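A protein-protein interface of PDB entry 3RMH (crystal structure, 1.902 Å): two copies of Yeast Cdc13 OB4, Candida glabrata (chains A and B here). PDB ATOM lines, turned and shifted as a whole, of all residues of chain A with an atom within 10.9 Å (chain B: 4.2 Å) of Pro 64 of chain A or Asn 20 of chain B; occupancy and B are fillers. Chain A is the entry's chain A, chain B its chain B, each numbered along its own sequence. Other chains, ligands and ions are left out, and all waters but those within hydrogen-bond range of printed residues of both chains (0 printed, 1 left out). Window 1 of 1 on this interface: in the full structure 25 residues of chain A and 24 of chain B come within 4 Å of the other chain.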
ATOM      1  N   ASN A  15      -7.329   7.753  -1.888  1.00  0.00           N
ATOM      2  CA  ASN A  15      -6.627   8.722  -1.073  1.00  0.00           C
ATOM      3  C   ASN A  15      -6.507  10.056  -1.799  1.00  0.00           C
ATOM      4  O   ASN A  15      -5.559  10.293  -2.540  1.00  0.00           O
ATOM      5  CB  ASN A  15      -5.250   8.173  -0.694  1.00  0.00           C
ATOM      6  CG  ASN A  15      -4.653   8.866   0.511  1.00  0.00           C
ATOM      7  OD1 ASN A  15      -4.999  10.005   0.821  1.00  0.00           O
ATOM      8  ND2 ASN A  15      -3.741   8.180   1.196  1.00  0.00           N
ATOM      9  N   ILE A  16      -7.499  10.912  -1.599  1.00  0.00           N
ATOM     10  CA  ILE A  16      -7.496  12.251  -2.172  1.00  0.00           C
ATOM     11  C   ILE A  16      -6.298  13.052  -1.693  1.00  0.00           C
ATOM     12  O   ILE A  16      -5.796  13.926  -2.403  1.00  0.00           O
ATOM     13  CB  ILE A  16      -8.790  12.988  -1.806  1.00  0.00           C
ATOM     14  CG1 ILE A  16      -9.927  12.476  -2.692  1.00  0.00           C
ATOM     15  CG2 ILE A  16      -8.613  14.517  -1.913  1.00  0.00           C
ATOM     16  CD1 ILE A  16     -11.281  12.978  -2.273  1.00  0.00           C
ATOM     17  N   SER A  17      -5.845  12.760  -0.484  1.00  0.00           N
ATOM     18  CA  SER A  17      -4.664  13.408   0.050  1.00  0.00           C
ATOM     19  C   SER A  17      -3.469  13.141  -0.861  1.00  0.00           C
ATOM     20  O   SER A  17      -2.691  14.044  -1.165  1.00  0.00           O
ATOM     21  CB  SER A  17      -4.378  12.889   1.455  1.00  0.00           C
ATOM     22  OG  SER A  17      -3.180  13.445   1.954  1.00  0.00           O
ATOM     23  N   GLN A  18      -3.329  11.898  -1.302  1.00  0.00           N
ATOM     24  CA  GLN A  18      -2.222  11.537  -2.181  1.00  0.00           C
ATOM     25  C   GLN A  18      -2.327  12.292  -3.493  1.00  0.00           C
ATOM     26  O   GLN A  18      -1.337  12.823  -3.989  1.00  0.00           O
ATOM     27  CB  GLN A  18      -2.216  10.036  -2.457  1.00  0.00           C
ATOM     28  CG  GLN A  18      -1.929   9.187  -1.235  1.00  0.00           C
ATOM     29  CD  GLN A  18      -2.015   7.699  -1.532  1.00  0.00           C
ATOM     30  OE1 GLN A  18      -1.308   6.896  -0.925  1.00  0.00           O
ATOM     31  NE2 GLN A  18      -2.884   7.325  -2.469  1.00  0.00           N
ATOM     32  N   LEU A  19      -3.528  12.335  -4.061  1.00  0.00           N
ATOM     33  CA  LEU A  19      -3.715  13.039  -5.320  1.00  0.00           C
ATOM     34  C   LEU A  19      -3.300  14.490  -5.161  1.00  0.00           C
ATOM     35  O   LEU A  19      -2.638  15.057  -6.039  1.00  0.00           O
ATOM     36  CB  LEU A  19      -5.164  12.965  -5.780  1.00  0.00           C
ATOM     37  CG  LEU A  19      -5.634  11.551  -6.121  1.00  0.00           C
ATOM     38  CD1 LEU A  19      -7.022  11.607  -6.715  1.00  0.00           C
ATOM     39  CD2 LEU A  19      -4.651  10.906  -7.089  1.00  0.00           C
ATOM     40  N   ASN A  20      -3.687  15.096  -4.043  1.00  0.00           N
ATOM     41  CA  ASN A  20      -3.380  16.517  -3.845  1.00  0.00           C
ATOM     42  C   ASN A  20      -1.892  16.816  -3.762  1.00  0.00           C
ATOM     43  O   ASN A  20      -1.484  17.977  -3.861  1.00  0.00           O
ATOM     44  CB  ASN A  20      -4.112  17.097  -2.626  1.00  0.00           C
ATOM     45  CG  ASN A  20      -5.539  17.494  -2.951  1.00  0.00           C
ATOM     46  OD1 ASN A  20      -5.835  17.926  -4.071  1.00  0.00           O
ATOM     47  ND2 ASN A  20      -6.433  17.346  -1.978  1.00  0.00           N
ATOM     48  N   HIS A  21      -1.086  15.775  -3.578  1.00  0.00           N
ATOM     49  CA  HIS A  21       0.367  15.944  -3.445  1.00  0.00           C
ATOM     50  C   HIS A  21       1.149  15.694  -4.735  1.00  0.00           C
ATOM     51  O   HIS A  21       2.315  16.070  -4.841  1.00  0.00           O
ATOM     52  CB  HIS A  21       0.918  15.039  -2.336  1.00  0.00           C
ATOM     53  CG  HIS A  21       0.757  15.606  -0.962  1.00  0.00           C
ATOM     54  ND1 HIS A  21       1.661  16.480  -0.404  1.00  0.00           N
ATOM     55  CD2 HIS A  21      -0.216  15.428  -0.029  1.00  0.00           C
ATOM     56  CE1 HIS A  21       1.262  16.818   0.809  1.00  0.00           C
ATOM     57  NE2 HIS A  21       0.124  16.193   1.057  1.00  0.00           N
ATOM     58  N   ILE A  37     -19.479  17.257  -1.597  1.00  0.00           N
ATOM     59  CA  ILE A  37     -19.860  18.022  -0.408  1.00  0.00           C
ATOM     60  C   ILE A  37     -20.101  19.502  -0.668  1.00  0.00           C
ATOM     61  O   ILE A  37     -20.595  20.214   0.204  1.00  0.00           O
ATOM     62  CB  ILE A  37     -18.825  17.877   0.727  1.00  0.00           C
ATOM     63  CG1 ILE A  37     -17.467  18.456   0.307  1.00  0.00           C
ATOM     64  CG2 ILE A  37     -18.709  16.425   1.158  1.00  0.00           C
ATOM     65  CD1 ILE A  37     -16.476  18.505   1.438  1.00  0.00           C
ATOM     66  N   ILE A  49     -16.465  21.244  -8.156  1.00  0.00           N
ATOM     67  CA  ILE A  49     -17.076  20.227  -7.310  1.00  0.00           C
ATOM     68  C   ILE A  49     -16.077  19.781  -6.250  1.00  0.00           C
ATOM     69  O   ILE A  49     -14.978  19.355  -6.575  1.00  0.00           O
ATOM     70  CB  ILE A  49     -17.512  19.033  -8.170  1.00  0.00           C
ATOM     71  CG1 ILE A  49     -18.476  19.515  -9.254  1.00  0.00           C
ATOM     72  CG2 ILE A  49     -18.142  17.931  -7.305  1.00  0.00           C
ATOM     73  CD1 ILE A  49     -18.878  18.430 -10.244  1.00  0.00           C
ATOM     74  N   LYS A  50     -16.446  19.898  -4.981  1.00  0.00           N
ATOM     75  CA  LYS A  50     -15.563  19.459  -3.912  1.00  0.00           C
ATOM     76  C   LYS A  50     -15.980  18.081  -3.426  1.00  0.00           C
ATOM     77  O   LYS A  50     -17.154  17.849  -3.130  1.00  0.00           O
ATOM     78  CB  LYS A  50     -15.542  20.473  -2.767  1.00  0.00           C
ATOM     79  CG  LYS A  50     -14.829  21.775  -3.187  1.00  0.00           C
ATOM     80  CD  LYS A  50     -14.741  22.800  -2.071  1.00  0.00           C
ATOM     81  CE  LYS A  50     -13.870  23.976  -2.527  1.00  0.00           C
ATOM     82  NZ  LYS A  50     -13.635  24.936  -1.422  1.00  0.00           N
ATOM     83  N   VAL A  51     -15.016  17.165  -3.386  1.00  0.00           N
ATOM     84  CA  VAL A  51     -15.287  15.795  -2.951  1.00  0.00           C
ATOM     85  C   VAL A  51     -14.336  15.340  -1.858  1.00  0.00           C
ATOM     86  O   VAL A  51     -13.212  15.841  -1.741  1.00  0.00           O
ATOM     87  CB  VAL A  51     -15.233  14.794  -4.134  1.00  0.00           C
ATOM     88  CG1 VAL A  51     -16.198  15.208  -5.227  1.00  0.00           C
ATOM     89  CG2 VAL A  51     -13.811  14.713  -4.705  1.00  0.00           C
ATOM     90  N   VAL A  52     -14.802  14.375  -1.066  1.00  0.00           N
ATOM     91  CA  VAL A  52     -14.032  13.776   0.012  1.00  0.00           C
ATOM     92  C   VAL A  52     -14.265  12.255   0.013  1.00  0.00           C
ATOM     93  O   VAL A  52     -15.300  11.784  -0.453  1.00  0.00           O
ATOM     94  CB  VAL A  52     -14.429  14.385   1.388  1.00  0.00           C
ATOM     95  CG1 VAL A  52     -14.133  15.867   1.410  1.00  0.00           C
ATOM     96  CG2 VAL A  52     -15.913  14.131   1.685  1.00  0.00           C
ATOM     97  N   ASN A  53     -13.285  11.495   0.498  1.00  0.00           N
ATOM     98  CA  ASN A  53     -13.414  10.043   0.600  1.00  0.00           C
ATOM     99  C   ASN A  53     -14.435   9.627   1.657  1.00  0.00           C
ATOM    100  O   ASN A  53     -15.103   8.607   1.507  1.00  0.00           O
ATOM    101  CB  ASN A  53     -12.068   9.376   0.912  1.00  0.00           C
ATOM    102  CG  ASN A  53     -11.113   9.368  -0.274  1.00  0.00           C
ATOM    103  OD1 ASN A  53     -10.031   9.954  -0.211  1.00  0.00           O
ATOM    104  ND2 ASN A  53     -11.493   8.674  -1.347  1.00  0.00           N
ATOM    105  N   TYR A  61     -13.732  17.544  11.657  1.00  0.00           N
ATOM    106  CA  TYR A  61     -13.614  18.511  10.565  1.00  0.00           C
ATOM    107  C   TYR A  61     -12.861  17.896   9.392  1.00  0.00           C
ATOM    108  O   TYR A  61     -12.142  16.911   9.561  1.00  0.00           O
ATOM    109  CB  TYR A  61     -12.847  19.757  11.041  1.00  0.00           C
ATOM    110  CG  TYR A  61     -13.614  20.626  12.018  1.00  0.00           C
ATOM    111  CD1 TYR A  61     -14.553  21.549  11.565  1.00  0.00           C
ATOM    112  CD2 TYR A  61     -13.389  20.535  13.387  1.00  0.00           C
ATOM    113  CE1 TYR A  61     -15.254  22.344  12.449  1.00  0.00           C
ATOM    114  CE2 TYR A  61     -14.097  21.331  14.285  1.00  0.00           C
ATOM    115  CZ  TYR A  61     -15.025  22.231  13.803  1.00  0.00           C
ATOM    116  OH  TYR A  61     -15.725  23.029  14.672  1.00  0.00           O
ATOM    117  N   VAL A  62     -13.040  18.476   8.206  1.00  0.00           N
ATOM    118  CA  VAL A  62     -12.293  18.079   7.020  1.00  0.00           C
ATOM    119  C   VAL A  62     -11.189  19.113   6.740  1.00  0.00           C
ATOM    120  O   VAL A  62     -11.472  20.292   6.523  1.00  0.00           O
ATOM    121  CB  VAL A  62     -13.198  17.977   5.772  1.00  0.00           C
ATOM    122  CG1 VAL A  62     -12.451  17.301   4.643  1.00  0.00           C
ATOM    123  CG2 VAL A  62     -14.476  17.194   6.089  1.00  0.00           C
ATOM    124  N   PRO A  63      -9.924  18.668   6.732  1.00  0.00           N
ATOM    125  CA  PRO A  63      -8.828  19.578   6.382  1.00  0.00           C
ATOM    126  C   PRO A  63      -8.729  19.700   4.865  1.00  0.00           C
ATOM    127  O   PRO A  63      -9.137  18.780   4.143  1.00  0.00           O
ATOM    128  CB  PRO A  63      -7.602  18.861   6.941  1.00  0.00           C
ATOM    129  CG  PRO A  63      -7.935  17.421   6.805  1.00  0.00           C
ATOM    130  CD  PRO A  63      -9.438  17.310   7.037  1.00  0.00           C
ATOM    131  N   PRO A  64      -8.196  20.825   4.374  1.00  0.00           N
ATOM    132  CA  PRO A  64      -8.148  21.089   2.934  1.00  0.00           C
ATOM    133  C   PRO A  64      -7.492  19.971   2.130  1.00  0.00           C
ATOM    134  O   PRO A  64      -7.902  19.717   1.004  1.00  0.00           O
ATOM    135  CB  PRO A  64      -7.285  22.361   2.845  1.00  0.00           C
ATOM    136  CG  PRO A  64      -7.530  23.052   4.130  1.00  0.00           C
ATOM    137  CD  PRO A  64      -7.650  21.947   5.158  1.00  0.00           C
ATOM    138  N   VAL A  65      -6.474  19.322   2.682  1.00  0.00           N
ATOM    139  CA  VAL A  65      -5.752  18.305   1.917  1.00  0.00           C
ATOM    140  C   VAL A  65      -6.625  17.090   1.620  1.00  0.00           C
ATOM    141  O   VAL A  65      -6.354  16.340   0.687  1.00  0.00           O
ATOM    142  CB  VAL A  65      -4.485  17.882   2.631  1.00  0.00           C
ATOM    143  N   ASP A  66      -7.674  16.896   2.407  1.00  0.00           N
ATOM    144  CA  ASP A  66      -8.588  15.773   2.181  1.00  0.00           C
ATOM    145  C   ASP A  66      -9.698  16.089   1.181  1.00  0.00           C
ATOM    146  O   ASP A  66     -10.571  15.254   0.918  1.00  0.00           O
ATOM    147  CB  ASP A  66      -9.201  15.311   3.504  1.00  0.00           C
ATOM    148  CG  ASP A  66      -8.232  14.510   4.342  1.00  0.00           C
ATOM    149  OD1 ASP A  66      -7.182  14.095   3.805  1.00  0.00           O
ATOM    150  OD2 ASP A  66      -8.522  14.285   5.535  1.00  0.00           O
ATOM    151  N   ILE A  67      -9.681  17.294   0.624  1.00  0.00           N
ATOM    152  CA  ILE A  67     -10.723  17.685  -0.316  1.00  0.00           C
ATOM    153  C   ILE A  67     -10.126  17.792  -1.696  1.00  0.00           C
ATOM    154  O   ILE A  67      -9.115  18.454  -1.870  1.00  0.00           O
ATOM    155  CB  ILE A  67     -11.336  19.042   0.083  1.00  0.00           C
ATOM    156  CG1 ILE A  67     -12.039  18.905   1.444  1.00  0.00           C
ATOM    157  CG2 ILE A  67     -12.324  19.531  -0.969  1.00  0.00           C
ATOM    158  CD1 ILE A  67     -12.274  20.236   2.155  1.00  0.00           C
ATOM    159  N   LEU A  68     -10.733  17.121  -2.670  1.00  0.00           N
ATOM    160  CA  LEU A  68     -10.314  17.285  -4.055  1.00  0.00           C
ATOM    161  C   LEU A  68     -11.259  18.257  -4.742  1.00  0.00           C
ATOM    162  O   LEU A  68     -12.475  18.061  -4.758  1.00  0.00           O
ATOM    163  CB  LEU A  68     -10.270  15.938  -4.792  1.00  0.00           C
ATOM    164  CG  LEU A  68      -9.536  15.958  -6.148  1.00  0.00           C
ATOM    165  CD1 LEU A  68      -8.031  16.054  -5.946  1.00  0.00           C
ATOM    166  CD2 LEU A  68      -9.884  14.723  -6.988  1.00  0.00           C
ATOM    167  N   GLU A  69     -10.712  19.326  -5.309  1.00  0.00           N
ATOM    168  CA  GLU A  69     -11.548  20.224  -6.088  1.00  0.00           C
ATOM    169  C   GLU A  69     -11.504  19.846  -7.567  1.00  0.00           C
ATOM    170  O   GLU A  69     -10.444  19.879  -8.205  1.00  0.00           O
ATOM    171  CB  GLU A  69     -11.140  21.684  -5.857  1.00  0.00           C
ATOM    172  CG  GLU A  69     -11.969  22.684  -6.650  1.00  0.00           C
ATOM    173  CD  GLU A  69     -12.017  24.057  -5.994  1.00  0.00           C
ATOM    174  OE1 GLU A  69     -12.957  24.827  -6.292  1.00  0.00           O
ATOM    175  OE2 GLU A  69     -11.120  24.365  -5.176  1.00  0.00           O
ATOM    176  N   VAL A  70     -12.667  19.500  -8.107  1.00  0.00           N
ATOM    177  CA  VAL A  70     -12.797  19.012  -9.469  1.00  0.00           C
ATOM    178  C   VAL A  70     -13.437  20.087 -10.334  1.00  0.00           C
ATOM    179  O   VAL A  70     -14.508  20.596 -10.006  1.00  0.00           O
ATOM    180  CB  VAL A  70     -13.674  17.727  -9.483  1.00  0.00           C
ATOM    181  CG1 VAL A  70     -13.835  17.195 -10.896  1.00  0.00           C
ATOM    182  CG2 VAL A  70     -13.054  16.672  -8.572  1.00  0.00           C
ATOM    183  N   TRP A 117      -7.620  19.301 -11.152  1.00  0.00           N
ATOM    184  CA  TRP A 117      -8.231  18.015 -11.433  1.00  0.00           C
ATOM    185  C   TRP A 117      -9.542  18.226 -12.172  1.00  0.00           C
ATOM    186  O   TRP A 117     -10.278  19.174 -11.884  1.00  0.00           O
ATOM    187  CB  TRP A 117      -8.448  17.266 -10.118  1.00  0.00           C
ATOM    188  CG  TRP A 117      -7.156  16.813  -9.530  1.00  0.00           C
ATOM    189  CD1 TRP A 117      -6.346  17.521  -8.685  1.00  0.00           C
ATOM    190  CD2 TRP A 117      -6.487  15.575  -9.797  1.00  0.00           C
ATOM    191  NE1 TRP A 117      -5.220  16.783  -8.393  1.00  0.00           N
ATOM    192  CE2 TRP A 117      -5.284  15.582  -9.053  1.00  0.00           C
ATOM    193  CE3 TRP A 117      -6.785  14.446 -10.569  1.00  0.00           C
ATOM    194  CZ2 TRP A 117      -4.389  14.510  -9.061  1.00  0.00           C
ATOM    195  CZ3 TRP A 117      -5.896  13.386 -10.581  1.00  0.00           C
ATOM    196  CH2 TRP A 117      -4.711  13.425  -9.829  1.00  0.00           C
ATOM    197  N   ILE B  16       3.188  24.944   4.226  1.00  0.00           N
ATOM    198  CA  ILE B  16       1.785  25.008   3.827  1.00  0.00           C
ATOM    199  C   ILE B  16       1.192  23.619   3.635  1.00  0.00           C
ATOM    200  O   ILE B  16       0.050  23.367   4.033  1.00  0.00           O
ATOM    201  CB  ILE B  16       1.619  25.864   2.558  1.00  0.00           C
ATOM    202  CG1 ILE B  16       1.502  27.338   2.949  1.00  0.00           C
ATOM    203  CG2 ILE B  16       0.403  25.417   1.741  1.00  0.00           C
ATOM    204  CD1 ILE B  16       1.487  28.280   1.755  1.00  0.00           C
ATOM    205  N   SER B  17       1.968  22.717   3.043  1.00  0.00           N
ATOM    206  CA  SER B  17       1.548  21.328   2.895  1.00  0.00           C
ATOM    207  C   SER B  17       1.174  20.720   4.247  1.00  0.00           C
ATOM    208  O   SER B  17       0.193  19.979   4.359  1.00  0.00           O
ATOM    209  CB  SER B  17       2.657  20.501   2.250  1.00  0.00           C
ATOM    210  OG  SER B  17       2.361  19.116   2.344  1.00  0.00           O
ATOM    211  N   GLN B  18       1.954  21.041   5.274  1.00  0.00           N
ATOM    212  CA  GLN B  18       1.679  20.558   6.622  1.00  0.00           C
ATOM    213  C   GLN B  18       0.430  21.208   7.211  1.00  0.00           C
ATOM    214  O   GLN B  18      -0.336  20.561   7.924  1.00  0.00           O
ATOM    215  CB  GLN B  18       2.882  20.789   7.545  1.00  0.00           C
ATOM    216  CG  GLN B  18       4.151  20.081   7.091  1.00  0.00           C
ATOM    217  CD  GLN B  18       5.274  20.154   8.117  1.00  0.00           C
ATOM    218  OE1 GLN B  18       5.195  20.902   9.094  1.00  0.00           O
ATOM    219  NE2 GLN B  18       6.324  19.367   7.898  1.00  0.00           N
ATOM    220  N   LEU B  19       0.220  22.482   6.905  1.00  0.00           N
ATOM    221  CA  LEU B  19      -0.934  23.205   7.416  1.00  0.00           C
ATOM    222  C   LEU B  19      -2.222  22.653   6.819  1.00  0.00           C
ATOM    223  O   LEU B  19      -3.244  22.561   7.501  1.00  0.00           O
ATOM    224  CB  LEU B  19      -0.820  24.695   7.104  1.00  0.00           C
ATOM    225  CG  LEU B  19       0.322  25.462   7.784  1.00  0.00           C
ATOM    226  CD1 LEU B  19       0.278  26.921   7.393  1.00  0.00           C
ATOM    227  CD2 LEU B  19       0.207  25.318   9.295  1.00  0.00           C
ATOM    228  N   ASN B  20      -2.170  22.288   5.540  1.00  0.00           N
ATOM    229  CA  ASN B  20      -3.356  21.756   4.861  1.00  0.00           C
ATOM    230  C   ASN B  20      -3.776  20.394   5.366  1.00  0.00           C
ATOM    231  O   ASN B  20      -4.884  19.939   5.084  1.00  0.00           O
ATOM    232  CB  ASN B  20      -3.141  21.688   3.346  1.00  0.00           C
ATOM    233  CG  ASN B  20      -3.390  23.015   2.674  1.00  0.00           C
ATOM    234  OD1 ASN B  20      -4.291  23.761   3.069  1.00  0.00           O
ATOM    235  ND2 ASN B  20      -2.588  23.324   1.655  1.00  0.00           N
ATOM    236  N   HIS B  21      -2.888  19.732   6.096  1.00  0.00           N
ATOM    237  CA  HIS B  21      -3.213  18.406   6.630  1.00  0.00           C
ATOM    238  C   HIS B  21      -3.781  18.441   8.045  1.00  0.00           C
ATOM    239  O   HIS B  21      -4.326  17.441   8.520  1.00  0.00           O
ATOM    240  CB  HIS B  21      -2.004  17.471   6.562  1.00  0.00           C
ATOM    241  CG  HIS B  21      -1.825  16.831   5.217  1.00  0.00           C
ATOM    242  ND1 HIS B  21      -2.311  15.585   4.925  1.00  0.00           N
ATOM    243  CD2 HIS B  21      -1.245  17.303   4.085  1.00  0.00           C
ATOM    244  CE1 HIS B  21      -2.022  15.293   3.660  1.00  0.00           C
ATOM    245  NE2 HIS B  21      -1.381  16.309   3.137  1.00  0.00           N
ATOM    246  N   LEU B  22      -3.655  19.583   8.715  1.00  0.00           N
ATOM    247  CA  LEU B  22      -4.104  19.687  10.109  1.00  0.00           C
ATOM    248  C   LEU B  22      -5.598  19.395  10.208  1.00  0.00           C
ATOM    249  O   LEU B  22      -6.427  20.156   9.701  1.00  0.00           O
ATOM    250  CB  LEU B  22      -3.787  21.065  10.688  1.00  0.00           C
ATOM    251  CG  LEU B  22      -2.317  21.378  10.983  1.00  0.00           C
ATOM    252  CD1 LEU B  22      -2.166  22.848  11.335  1.00  0.00           C
ATOM    253  CD2 LEU B  22      -1.770  20.506  12.107  1.00  0.00           C
ATOM    254  N   PRO B  64      -2.185  20.978  -5.500  1.00  0.00           N
ATOM    255  CA  PRO B  64      -3.128  21.637  -4.595  1.00  0.00           C
ATOM    256  C   PRO B  64      -2.671  21.667  -3.144  1.00  0.00           C
ATOM    257  O   PRO B  64      -2.974  22.622  -2.436  1.00  0.00           O
ATOM    258  CB  PRO B  64      -4.397  20.788  -4.738  1.00  0.00           C
ATOM    259  CG  PRO B  64      -4.309  20.247  -6.128  1.00  0.00           C
ATOM    260  CD  PRO B  64      -2.843  19.966  -6.342  1.00  0.00           C
ATOM    261  N   VAL B  65      -1.953  20.646  -2.696  1.00  0.00           N
ATOM    262  CA  VAL B  65      -1.590  20.590  -1.281  1.00  0.00           C
ATOM    263  C   VAL B  65      -0.575  21.666  -0.909  1.00  0.00           C
ATOM    264  O   VAL B  65      -0.411  21.985   0.268  1.00  0.00           O
ATOM    265  CB  VAL B  65      -1.069  19.218  -0.904  1.00  0.00           C
ATOM    266  N   ILE B  67      -0.781  24.753  -1.804  1.00  0.00           N
ATOM    267  CA  ILE B  67      -1.477  26.024  -1.872  1.00  0.00           C
ATOM    268  C   ILE B  67      -2.381  26.190  -0.659  1.00  0.00           C
ATOM    269  O   ILE B  67      -3.189  25.318  -0.367  1.00  0.00           O
ATOM    270  CB  ILE B  67      -2.343  26.093  -3.144  1.00  0.00           C
ATOM    271  CG1 ILE B  67      -1.440  26.074  -4.394  1.00  0.00           C
ATOM    272  CG2 ILE B  67      -3.206  27.357  -3.143  1.00  0.00           C
ATOM    273  CD1 ILE B  67      -2.201  25.754  -5.690  1.00  0.00           C
ATOM    274  N   LEU B  68      -2.246  27.314   0.041  1.00  0.00           N
ATOM    275  CA  LEU B  68      -3.137  27.619   1.151  1.00  0.00           C
ATOM    276  C   LEU B  68      -4.178  28.600   0.638  1.00  0.00           C
ATOM    277  O   LEU B  68      -3.842  29.640   0.060  1.00  0.00           O
ATOM    278  CB  LEU B  68      -2.355  28.210   2.332  1.00  0.00           C
ATOM    279  CG  LEU B  68      -3.087  28.145   3.686  1.00  0.00           C
ATOM    280  CD1 LEU B  68      -3.069  26.708   4.222  1.00  0.00           C
ATOM    281  CD2 LEU B  68      -2.439  29.071   4.698  1.00  0.00           C
ATOM    282  N   ILE B 115     -12.481  22.953   7.285  1.00  0.00           N
ATOM    283  CA  ILE B 115     -11.604  23.929   7.922  1.00  0.00           C
ATOM    284  C   ILE B 115     -11.207  24.965   6.876  1.00  0.00           C
ATOM    285  O   ILE B 115     -10.814  24.616   5.767  1.00  0.00           O
ATOM    286  CB  ILE B 115     -10.360  23.265   8.533  1.00  0.00           C
ATOM    287  CG1 ILE B 115     -10.747  22.545   9.825  1.00  0.00           C
ATOM    288  CG2 ILE B 115      -9.270  24.319   8.827  1.00  0.00           C
ATOM    289  CD1 ILE B 115      -9.681  21.608  10.346  1.00  0.00           C
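Ser 17 of chain A touches His 21 of chain B, and with the chains exchanged His 21 of chain A touches Ser 17 of chain B.
Asn 20 of chain A touches Pro 64 of chain B, and with the chains exchanged Pro 64 of chain A touches Asn 20 of chain B.
Asn 20 of chain A touches Val 65 of chain B, and with the chains exchanged Val 65 of chain A touches Asn 20 of chain B.
His 21 of chain B touches its own counterpart, His 21 of chain A.
10 positions are printed for both chains.
Of the 15 pairs that touch across the chains among the printed residues, 9 have their exchanged pair printed and touching as well.
Among the printed residues, merely in contact across the chains: Ser 17 of chain A with His 21 of chain B (2.8 Å), His 21 of chain A with Ser 17 of chain B (3.0 Å), Pro 63 of chain A with Leu 22 of chain B (3.3 Å), Pro 64 of chain A with Asn 20 of chain B (3.3 Å), Pro 63 of chain A with Asn 20 of chain B (3.5 Å), Val 65 of chain A with His 21 of chain B (3.5 Å), Tyr 61 of chain A with Ile 115 of chain B (3.7 Å), His 21 of chain A with Val 65 of chain B (3.8 Å), Pro 63 of chain A with His 21 of chain B (3.9 Å) and Pro 64 of chain A with Ile 115 of chain B (3.99 Å).
O of Asn 20 of chain A lies within hydrogen-bond range of N of Val 65 of chain B, at 2.9 Å.
A ring nitrogen (NE2) of His 21 of chain B lies within hydrogen-bond range of a ring nitrogen (NE2) of His 21 of chain A (2.6 Å).
N of Ile 115 of chain B sits at hydrogen-bond distance from O of Val 62 of chain A, at 2.9 Å.
The backbone carbonyl oxygen (O) of Asn 20 of chain B lies within hydrogen-bond range of the backbone NH (N) of Val 65 of chain A, 2.9 Å away.
The backbone carbonyl oxygen (O) of Asn 20 of chain A lies close to the backbone nitrogen (N) of Pro 64 of chain B, at 3.5 Å.
Printed residues of chain B within 4 Å of Pro 64 of chain A: Asn 20 and Ile 115.
Asn 20 of chain B touches three residues of chain A.
No residue of chain A comes within 4 Å of Ile 16 of chain B.
Ser 17 of chain B touches just one residue of chain A: His 21 (3.0 Å).
No residue of chain A comes within 4 Å of Leu 19 of chain B.
Leu 22 of chain B touches one residue of chain A.
Val 65 of chain B touches two residues of chain A.
Printed residues of chain A within 4 Å of Pro 64 of chain B: Asn 20.
Printed residues of chain B within 4 Å of Pro 63 of chain A: Asn 20 (3.5 Å), His 21 (3.9 Å) and Leu 22 (3.3 Å).
Of the printed residues of chain B, Val 65 of chain A touches Asn 20 and His 21.
Of the printed residues of chain B, Ser 17 of chain A touches His 21.
Asn 15 of chain A touches none of the printed residues of chain B.
Ile 67 of chain A touches none of the printed residues of chain B.
The nearest printed residue of chain B that does not touch Pro 64 of chain A is Leu 19 of chain B (5.0 Å).
The nearest residue of chain A that does not touch Asn 20 of chain B is Asp 66 of chain A (4.9 Å).
The nearest printed residue of chain B that does not touch Val 65 of chain A is Val 65 of chain B (5.1 Å).
The side-chain amide oxygen of Asn 15 of chain A lies close to the backbone NH of Ser 17 of chain A (3.2 Å).
The side-chain amide nitrogen (ND2) of Asn 20 of chain A lies within hydrogen-bond range of the backbone carbonyl oxygen (O) of Val 65 of chain A (2.8 Å).
The backbone carbonyl oxygen of Ile 67 of chain A is in hydrogen-bond range of the side-chain amide nitrogen of Asn 20 of chain A.
The side-chain amide nitrogen (ND2) of Asn 20 of chain B sits at hydrogen-bond distance from the backbone carbonyl oxygen (O) of Val 65 of chain B.
The backbone carbonyl oxygen of Ile 67 of chain B is in hydrogen-bond range of the side-chain amide nitrogen of Asn 20 of chain B (2.9 Å).
Of the 12 printed residues of chain B, 7 touch a printed residue of chain A.
Among the printed residues, 15 pairs touch across the chains.
Among the printed residues, no Asp or Glu carboxylate lies within 4 Å of a Lys or Arg side-chain nitrogen of the other chain.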
